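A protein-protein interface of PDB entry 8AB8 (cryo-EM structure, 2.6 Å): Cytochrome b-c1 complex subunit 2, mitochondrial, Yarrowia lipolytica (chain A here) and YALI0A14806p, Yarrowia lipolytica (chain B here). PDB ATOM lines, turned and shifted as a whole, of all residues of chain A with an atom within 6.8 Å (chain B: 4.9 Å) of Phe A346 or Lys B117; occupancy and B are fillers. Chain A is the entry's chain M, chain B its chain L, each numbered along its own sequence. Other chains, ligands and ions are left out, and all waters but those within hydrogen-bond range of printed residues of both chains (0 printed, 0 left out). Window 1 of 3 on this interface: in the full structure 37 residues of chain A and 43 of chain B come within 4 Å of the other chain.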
ATOM      1  N   TYR A 341     -11.612   0.371 -33.703  1.00  0.00           N
ATOM      2  CA  TYR A 341     -12.551   0.558 -32.619  1.00  0.00           C
ATOM      3  C   TYR A 341     -12.188   1.811 -31.833  1.00  0.00           C
ATOM      4  O   TYR A 341     -13.072   2.565 -31.433  1.00  0.00           O
ATOM      5  CB  TYR A 341     -12.499  -0.648 -31.687  1.00  0.00           C
ATOM      6  CG  TYR A 341     -13.258  -0.468 -30.401  1.00  0.00           C
ATOM      7  CD1 TYR A 341     -14.631  -0.262 -30.409  1.00  0.00           C
ATOM      8  CD2 TYR A 341     -12.614  -0.533 -29.174  1.00  0.00           C
ATOM      9  CE1 TYR A 341     -15.343  -0.116 -29.229  1.00  0.00           C
ATOM     10  CE2 TYR A 341     -13.312  -0.388 -27.985  1.00  0.00           C
ATOM     11  CZ  TYR A 341     -14.682  -0.179 -28.013  1.00  0.00           C
ATOM     12  OH  TYR A 341     -15.378  -0.038 -26.848  1.00  0.00           O
ATOM     13  N   ALA A 342     -10.885   1.985 -31.594  1.00  0.00           N
ATOM     14  CA  ALA A 342     -10.394   3.096 -30.801  1.00  0.00           C
ATOM     15  C   ALA A 342     -10.629   4.411 -31.538  1.00  0.00           C
ATOM     16  O   ALA A 342     -11.183   5.338 -30.958  1.00  0.00           O
ATOM     17  CB  ALA A 342      -8.943   2.906 -30.448  1.00  0.00           C
ATOM     18  N   LYS A 343     -10.218   4.473 -32.810  1.00  0.00           N
ATOM     19  CA  LYS A 343     -10.384   5.677 -33.609  1.00  0.00           C
ATOM     20  C   LYS A 343     -11.865   5.999 -33.791  1.00  0.00           C
ATOM     21  O   LYS A 343     -12.230   7.173 -33.853  1.00  0.00           O
ATOM     22  CB  LYS A 343      -9.667   5.576 -34.958  1.00  0.00           C
ATOM     23  CG  LYS A 343      -8.150   5.505 -34.870  1.00  0.00           C
ATOM     24  CD  LYS A 343      -7.457   6.364 -35.892  1.00  0.00           C
ATOM     25  CE  LYS A 343      -7.205   5.650 -37.201  1.00  0.00           C
ATOM     26  NZ  LYS A 343      -6.847   6.609 -38.274  1.00  0.00           N
ATOM     27  N   SER A 344     -12.718   4.967 -33.819  1.00  0.00           N
ATOM     28  CA  SER A 344     -14.132   5.205 -34.063  1.00  0.00           C
ATOM     29  C   SER A 344     -14.853   5.678 -32.805  1.00  0.00           C
ATOM     30  O   SER A 344     -15.705   6.551 -32.916  1.00  0.00           O
ATOM     31  CB  SER A 344     -14.819   4.032 -34.710  1.00  0.00           C
ATOM     32  OG  SER A 344     -14.898   2.938 -33.809  1.00  0.00           O
ATOM     33  N   LYS A 345     -14.557   5.076 -31.641  1.00  0.00           N
ATOM     34  CA  LYS A 345     -15.130   5.507 -30.371  1.00  0.00           C
ATOM     35  C   LYS A 345     -14.786   6.972 -30.125  1.00  0.00           C
ATOM     36  O   LYS A 345     -15.625   7.749 -29.680  1.00  0.00           O
ATOM     37  CB  LYS A 345     -14.481   4.764 -29.204  1.00  0.00           C
ATOM     38  CG  LYS A 345     -15.413   3.932 -28.346  1.00  0.00           C
ATOM     39  CD  LYS A 345     -15.036   3.955 -26.881  1.00  0.00           C
ATOM     40  CE  LYS A 345     -13.886   3.026 -26.549  1.00  0.00           C
ATOM     41  NZ  LYS A 345     -13.959   2.558 -25.145  1.00  0.00           N
ATOM     42  N   PHE A 346     -13.527   7.323 -30.402  1.00  0.00           N
ATOM     43  CA  PHE A 346     -13.061   8.680 -30.207  1.00  0.00           C
ATOM     44  C   PHE A 346     -13.820   9.635 -31.120  1.00  0.00           C
ATOM     45  O   PHE A 346     -14.223  10.701 -30.677  1.00  0.00           O
ATOM     46  CB  PHE A 346     -11.565   8.793 -30.482  1.00  0.00           C
ATOM     47  CG  PHE A 346     -11.028  10.182 -30.258  1.00  0.00           C
ATOM     48  CD1 PHE A 346     -10.903  10.705 -28.975  1.00  0.00           C
ATOM     49  CD2 PHE A 346     -10.657  10.973 -31.334  1.00  0.00           C
ATOM     50  CE1 PHE A 346     -10.414  11.990 -28.775  1.00  0.00           C
ATOM     51  CE2 PHE A 346     -10.158  12.254 -31.133  1.00  0.00           C
ATOM     52  CZ  PHE A 346     -10.044  12.763 -29.856  1.00  0.00           C
ATOM     53  N   ALA A 347     -13.982   9.259 -32.391  1.00  0.00           N
ATOM     54  CA  ALA A 347     -14.665  10.135 -33.328  1.00  0.00           C
ATOM     55  C   ALA A 347     -16.102  10.368 -32.866  1.00  0.00           C
ATOM     56  O   ALA A 347     -16.605  11.485 -32.956  1.00  0.00           O
ATOM     57  CB  ALA A 347     -14.601   9.573 -34.725  1.00  0.00           C
ATOM     58  N   ALA A 348     -16.739   9.316 -32.340  1.00  0.00           N
ATOM     59  CA  ALA A 348     -18.114   9.421 -31.878  1.00  0.00           C
ATOM     60  C   ALA A 348     -18.193  10.383 -30.700  1.00  0.00           C
ATOM     61  O   ALA A 348     -19.147  11.151 -30.603  1.00  0.00           O
ATOM     62  CB  ALA A 348     -18.656   8.064 -31.508  1.00  0.00           C
ATOM     63  N   ALA A 349     -17.186  10.320 -29.815  1.00  0.00           N
ATOM     64  CA  ALA A 349     -17.190  11.087 -28.581  1.00  0.00           C
ATOM     65  C   ALA A 349     -17.090  12.569 -28.908  1.00  0.00           C
ATOM     66  O   ALA A 349     -17.914  13.348 -28.448  1.00  0.00           O
ATOM     67  CB  ALA A 349     -16.090  10.636 -27.654  1.00  0.00           C
ATOM     68  N   GLU A 350     -16.134  12.929 -29.761  1.00  0.00           N
ATOM     69  CA  GLU A 350     -15.892  14.326 -30.079  1.00  0.00           C
ATOM     70  C   GLU A 350     -17.042  14.916 -30.902  1.00  0.00           C
ATOM     71  O   GLU A 350     -17.266  16.126 -30.853  1.00  0.00           O
ATOM     72  CB  GLU A 350     -14.508  14.495 -30.704  1.00  0.00           C
ATOM     73  CG  GLU A 350     -14.391  13.876 -32.082  1.00  0.00           C
ATOM     74  CD  GLU A 350     -12.994  13.788 -32.663  1.00  0.00           C
ATOM     75  OE1 GLU A 350     -12.755  12.846 -33.449  1.00  0.00           O
ATOM     76  OE2 GLU A 350     -12.168  14.675 -32.360  1.00  0.00           O
ATOM     77  N   ALA A 351     -17.790  14.068 -31.625  1.00  0.00           N
ATOM     78  CA  ALA A 351     -18.964  14.522 -32.359  1.00  0.00           C
ATOM     79  C   ALA A 351     -20.098  14.876 -31.398  1.00  0.00           C
ATOM     80  O   ALA A 351     -20.832  15.837 -31.627  1.00  0.00           O
ATOM     81  CB  ALA A 351     -19.392  13.495 -33.376  1.00  0.00           C
ATOM     82  N   GLU A 353     -19.598  15.969 -28.518  1.00  0.00           N
ATOM     83  CA  GLU A 353     -19.116  17.076 -27.707  1.00  0.00           C
ATOM     84  C   GLU A 353     -19.297  18.396 -28.450  1.00  0.00           C
ATOM     85  O   GLU A 353     -19.839  19.340 -27.875  1.00  0.00           O
ATOM     86  CB  GLU A 353     -17.675  16.846 -27.257  1.00  0.00           C
ATOM     87  CG  GLU A 353     -17.564  15.914 -26.060  1.00  0.00           C
ATOM     88  CD  GLU A 353     -16.455  14.870 -26.146  1.00  0.00           C
ATOM     89  OE1 GLU A 353     -15.414  15.170 -26.761  1.00  0.00           O
ATOM     90  OE2 GLU A 353     -16.661  13.729 -25.655  1.00  0.00           O
ATOM     91  N   PRO A 375     -21.164   7.201 -27.275  1.00  0.00           N
ATOM     92  CA  PRO A 375     -19.784   6.815 -27.586  1.00  0.00           C
ATOM     93  C   PRO A 375     -19.254   5.625 -26.786  1.00  0.00           C
ATOM     94  O   PRO A 375     -18.433   4.864 -27.289  1.00  0.00           O
ATOM     95  CB  PRO A 375     -18.960   8.089 -27.341  1.00  0.00           C
ATOM     96  CG  PRO A 375     -19.886   9.004 -26.571  1.00  0.00           C
ATOM     97  CD  PRO A 375     -21.284   8.645 -27.031  1.00  0.00           C
ATOM     98  N   VAL A 378     -20.407   2.225 -28.602  1.00  0.00           N
ATOM     99  CA  VAL A 378     -19.946   1.991 -29.957  1.00  0.00           C
ATOM    100  C   VAL A 378     -19.427   0.558 -30.051  1.00  0.00           C
ATOM    101  O   VAL A 378     -18.606   0.135 -29.239  1.00  0.00           O
ATOM    102  CB  VAL A 378     -18.900   3.057 -30.338  1.00  0.00           C
ATOM    103  CG1 VAL A 378     -17.978   2.663 -31.485  1.00  0.00           C
ATOM    104  CG2 VAL A 378     -19.562   4.396 -30.606  1.00  0.00           C
ATOM    105  N   THR B  51     -14.058  12.778 -23.192  1.00  0.00           N
ATOM    106  CA  THR B  51     -12.761  12.959 -23.813  1.00  0.00           C
ATOM    107  C   THR B  51     -11.939  13.895 -22.935  1.00  0.00           C
ATOM    108  O   THR B  51     -12.507  14.724 -22.238  1.00  0.00           O
ATOM    109  CB  THR B  51     -13.003  13.433 -25.250  1.00  0.00           C
ATOM    110  OG1 THR B  51     -12.867  12.292 -26.096  1.00  0.00           O
ATOM    111  CG2 THR B  51     -12.165  14.610 -25.683  1.00  0.00           C
ATOM    112  N   ALA B  52     -10.608  13.790 -22.999  1.00  0.00           N
ATOM    113  CA  ALA B  52      -9.733  14.606 -22.171  1.00  0.00           C
ATOM    114  C   ALA B  52      -8.611  15.205 -23.016  1.00  0.00           C
ATOM    115  O   ALA B  52      -8.140  14.568 -23.942  1.00  0.00           O
ATOM    116  CB  ALA B  52      -9.191  13.746 -21.068  1.00  0.00           C
ATOM    117  N   THR B  53      -8.217  16.446 -22.717  1.00  0.00           N
ATOM    118  CA  THR B  53      -7.025  17.028 -23.314  1.00  0.00           C
ATOM    119  C   THR B  53      -5.966  17.192 -22.231  1.00  0.00           C
ATOM    120  O   THR B  53      -6.121  18.041 -21.362  1.00  0.00           O
ATOM    121  CB  THR B  53      -7.345  18.371 -23.987  1.00  0.00           C
ATOM    122  OG1 THR B  53      -8.367  18.131 -24.957  1.00  0.00           O
ATOM    123  CG2 THR B  53      -6.140  18.998 -24.652  1.00  0.00           C
ATOM    124  N   MET B  99      -4.048   4.616 -29.642  1.00  0.00           N
ATOM    125  CA  MET B  99      -4.730   5.369 -28.600  1.00  0.00           C
ATOM    126  C   MET B  99      -6.155   5.659 -29.056  1.00  0.00           C
ATOM    127  O   MET B  99      -7.108   5.460 -28.301  1.00  0.00           O
ATOM    128  CB  MET B  99      -4.085   6.743 -28.416  1.00  0.00           C
ATOM    129  CG  MET B  99      -3.169   6.956 -27.261  1.00  0.00           C
ATOM    130  SD  MET B  99      -3.315   8.723 -26.758  1.00  0.00           S
ATOM    131  CE  MET B  99      -3.565   9.588 -28.318  1.00  0.00           C
ATOM    132  N   GLY B 100      -6.274   6.180 -30.286  1.00  0.00           N
ATOM    133  CA  GLY B 100      -7.561   6.601 -30.809  1.00  0.00           C
ATOM    134  C   GLY B 100      -7.644   8.109 -31.031  1.00  0.00           C
ATOM    135  O   GLY B 100      -8.330   8.557 -31.951  1.00  0.00           O
ATOM    136  N   GLY B 101      -6.953   8.884 -30.184  1.00  0.00           N
ATOM    137  CA  GLY B 101      -6.999  10.332 -30.282  1.00  0.00           C
ATOM    138  C   GLY B 101      -5.855  10.859 -31.138  1.00  0.00           C
ATOM    139  O   GLY B 101      -5.351  10.153 -32.003  1.00  0.00           O
ATOM    140  N   HIS B 102      -5.456  12.106 -30.892  1.00  0.00           N
ATOM    141  CA  HIS B 102      -4.375  12.695 -31.661  1.00  0.00           C
ATOM    142  C   HIS B 102      -3.466  13.501 -30.745  1.00  0.00           C
ATOM    143  O   HIS B 102      -3.811  13.779 -29.596  1.00  0.00           O
ATOM    144  CB  HIS B 102      -4.935  13.550 -32.803  1.00  0.00           C
ATOM    145  CG  HIS B 102      -5.823  14.637 -32.310  1.00  0.00           C
ATOM    146  ND1 HIS B 102      -7.170  14.438 -32.082  1.00  0.00           N
ATOM    147  CD2 HIS B 102      -5.560  15.914 -31.965  1.00  0.00           C
ATOM    148  CE1 HIS B 102      -7.708  15.555 -31.636  1.00  0.00           C
ATOM    149  NE2 HIS B 102      -6.741  16.481 -31.562  1.00  0.00           N
ATOM    150  N   TYR B 115       0.223  18.807 -26.768  1.00  0.00           N
ATOM    151  CA  TYR B 115      -0.894  18.209 -26.061  1.00  0.00           C
ATOM    152  C   TYR B 115      -1.418  16.979 -26.786  1.00  0.00           C
ATOM    153  O   TYR B 115      -1.093  16.739 -27.943  1.00  0.00           O
ATOM    154  CB  TYR B 115      -1.982  19.242 -25.781  1.00  0.00           C
ATOM    155  CG  TYR B 115      -2.724  19.726 -26.996  1.00  0.00           C
ATOM    156  CD1 TYR B 115      -3.847  19.058 -27.465  1.00  0.00           C
ATOM    157  CD2 TYR B 115      -2.329  20.876 -27.656  1.00  0.00           C
ATOM    158  CE1 TYR B 115      -4.550  19.516 -28.566  1.00  0.00           C
ATOM    159  CE2 TYR B 115      -3.017  21.346 -28.764  1.00  0.00           C
ATOM    160  CZ  TYR B 115      -4.137  20.667 -29.215  1.00  0.00           C
ATOM    161  OH  TYR B 115      -4.815  21.116 -30.312  1.00  0.00           O
ATOM    162  N   ALA B 116      -2.277  16.242 -26.083  1.00  0.00           N
ATOM    163  CA  ALA B 116      -2.838  15.003 -26.586  1.00  0.00           C
ATOM    164  C   ALA B 116      -4.312  14.970 -26.220  1.00  0.00           C
ATOM    165  O   ALA B 116      -4.646  15.031 -25.041  1.00  0.00           O
ATOM    166  CB  ALA B 116      -2.115  13.849 -25.949  1.00  0.00           C
ATOM    167  N   LYS B 117      -5.176  14.893 -27.234  1.00  0.00           N
ATOM    168  CA  LYS B 117      -6.590  14.688 -26.984  1.00  0.00           C
ATOM    169  C   LYS B 117      -6.880  13.196 -27.097  1.00  0.00           C
ATOM    170  O   LYS B 117      -6.432  12.550 -28.037  1.00  0.00           O
ATOM    171  CB  LYS B 117      -7.428  15.519 -27.955  1.00  0.00           C
ATOM    172  CG  LYS B 117      -8.864  15.749 -27.532  1.00  0.00           C
ATOM    173  CD  LYS B 117      -9.548  16.722 -28.474  1.00  0.00           C
ATOM    174  CE  LYS B 117     -11.049  16.846 -28.310  1.00  0.00           C
ATOM    175  NZ  LYS B 117     -11.445  17.829 -27.266  1.00  0.00           N
ATOM    176  N   SER B 118      -7.599  12.653 -26.116  1.00  0.00           N
ATOM    177  CA  SER B 118      -7.836  11.223 -26.098  1.00  0.00           C
ATOM    178  C   SER B 118      -9.203  10.915 -25.504  1.00  0.00           C
ATOM    179  O   SER B 118     -10.026  11.809 -25.302  1.00  0.00           O
ATOM    180  CB  SER B 118      -6.747  10.512 -25.336  1.00  0.00           C
ATOM    181  OG  SER B 118      -6.713  10.965 -23.993  1.00  0.00           O
ATOM    182  N   PHE B 119      -9.414   9.622 -25.251  1.00  0.00           N
ATOM    183  CA  PHE B 119     -10.535   9.123 -24.483  1.00  0.00           C
ATOM    184  C   PHE B 119     -10.193   9.205 -22.997  1.00  0.00           C
ATOM    185  O   PHE B 119      -9.037   9.408 -22.647  1.00  0.00           O
ATOM    186  CB  PHE B 119     -10.920   7.722 -24.970  1.00  0.00           C
ATOM    187  CG  PHE B 119     -12.408   7.532 -24.914  1.00  0.00           C
ATOM    188  CD1 PHE B 119     -13.227   8.151 -25.846  1.00  0.00           C
ATOM    189  CD2 PHE B 119     -12.995   6.839 -23.865  1.00  0.00           C
ATOM    190  CE1 PHE B 119     -14.607   8.031 -25.759  1.00  0.00           C
ATOM    191  CE2 PHE B 119     -14.377   6.727 -23.775  1.00  0.00           C
ATOM    192  CZ  PHE B 119     -15.180   7.328 -24.721  1.00  0.00           C
ATOM    193  N   THR B 400     -12.815  20.858 -24.445  1.00  0.00           N
ATOM    194  CA  THR B 400     -11.737  20.554 -23.520  1.00  0.00           C
ATOM    195  C   THR B 400     -10.430  21.197 -23.974  1.00  0.00           C
ATOM    196  O   THR B 400      -9.613  21.561 -23.136  1.00  0.00           O
ATOM    197  CB  THR B 400     -11.578  19.043 -23.315  1.00  0.00           C
ATOM    198  OG1 THR B 400     -11.067  18.486 -24.523  1.00  0.00           O
ATOM    199  CG2 THR B 400     -12.864  18.346 -22.932  1.00  0.00           C
ATOM    200  N   THR B 401     -10.229  21.318 -25.290  1.00  0.00           N
ATOM    201  CA  THR B 401      -8.982  21.875 -25.786  1.00  0.00           C
ATOM    202  C   THR B 401      -8.925  23.368 -25.485  1.00  0.00           C
ATOM    203  O   THR B 401      -7.850  23.881 -25.189  1.00  0.00           O
ATOM    204  CB  THR B 401      -8.723  21.540 -27.260  1.00  0.00           C
ATOM    205  OG1 THR B 401      -8.764  20.122 -27.367  1.00  0.00           O
ATOM    206  CG2 THR B 401      -7.361  21.994 -27.740  1.00  0.00           C
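O of Ser B118 is in hydrogen-bond range of OG1 of Thr B51 (3.0 Å). O of Ala B52 lies within hydrogen-bond range of N of Ser B118. The backbone carbonyl oxygen (O) of His B102 is in hydrogen-bond range of the backbone NH (N) of Lys B117, at 2.9 Å. NZ of Lys B117 lies within hydrogen-bond range of OG1 of Thr B400 (2.8 Å).
CB of Ala A342 touches O of Met B99, at 3.8 Å. Ala A342 touches Gly B100 (O to CA, 3.8 Å). CA of Lys A343 touches O of Gly B100, at 3.9 Å. OG1 of Thr B51 touches CE1 of Phe A346, 3.6 Å away. Phe A346 touches Gly B100. CA of Gly B101 touches CE2 of Phe A346, at 3.8 Å. Phe A346 touches His B102. CZ of Phe A346 touches CG of Lys B117, 3.96 Å away. Ala A349 touches Phe B119. OE1 of Glu A353 touches CB of Thr B51, at 3.3 Å.
Of chain B, only Thr B51, Gly B100, Gly B101, His B102, Lys B117 and Ser B118 come within 4 Å of Phe A346. Of the printed residues of chain A, His B102 touches Phe A346. Of the printed residues of chain A, Ser B118 touches Phe A346 (3.5 Å). The nearest residue of chain B that does not touch Phe A346 is Phe B119 (4.2 Å).
Hydrophobic or aromatic side chains of chain A within 4 Å of the printed part of chain B: Ala A342, Phe A346 and Ala A349. Hydrophobic or aromatic side chains of chain B within 4 Å of the printed part of chain A: His B102 and Phe B119. Among the printed residues, 12 pairs touch across the chains. Among the printed residues, no Asp or Glu carboxylate lies within 4 Å of a Lys or Arg side-chain nitrogen of the other chain.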
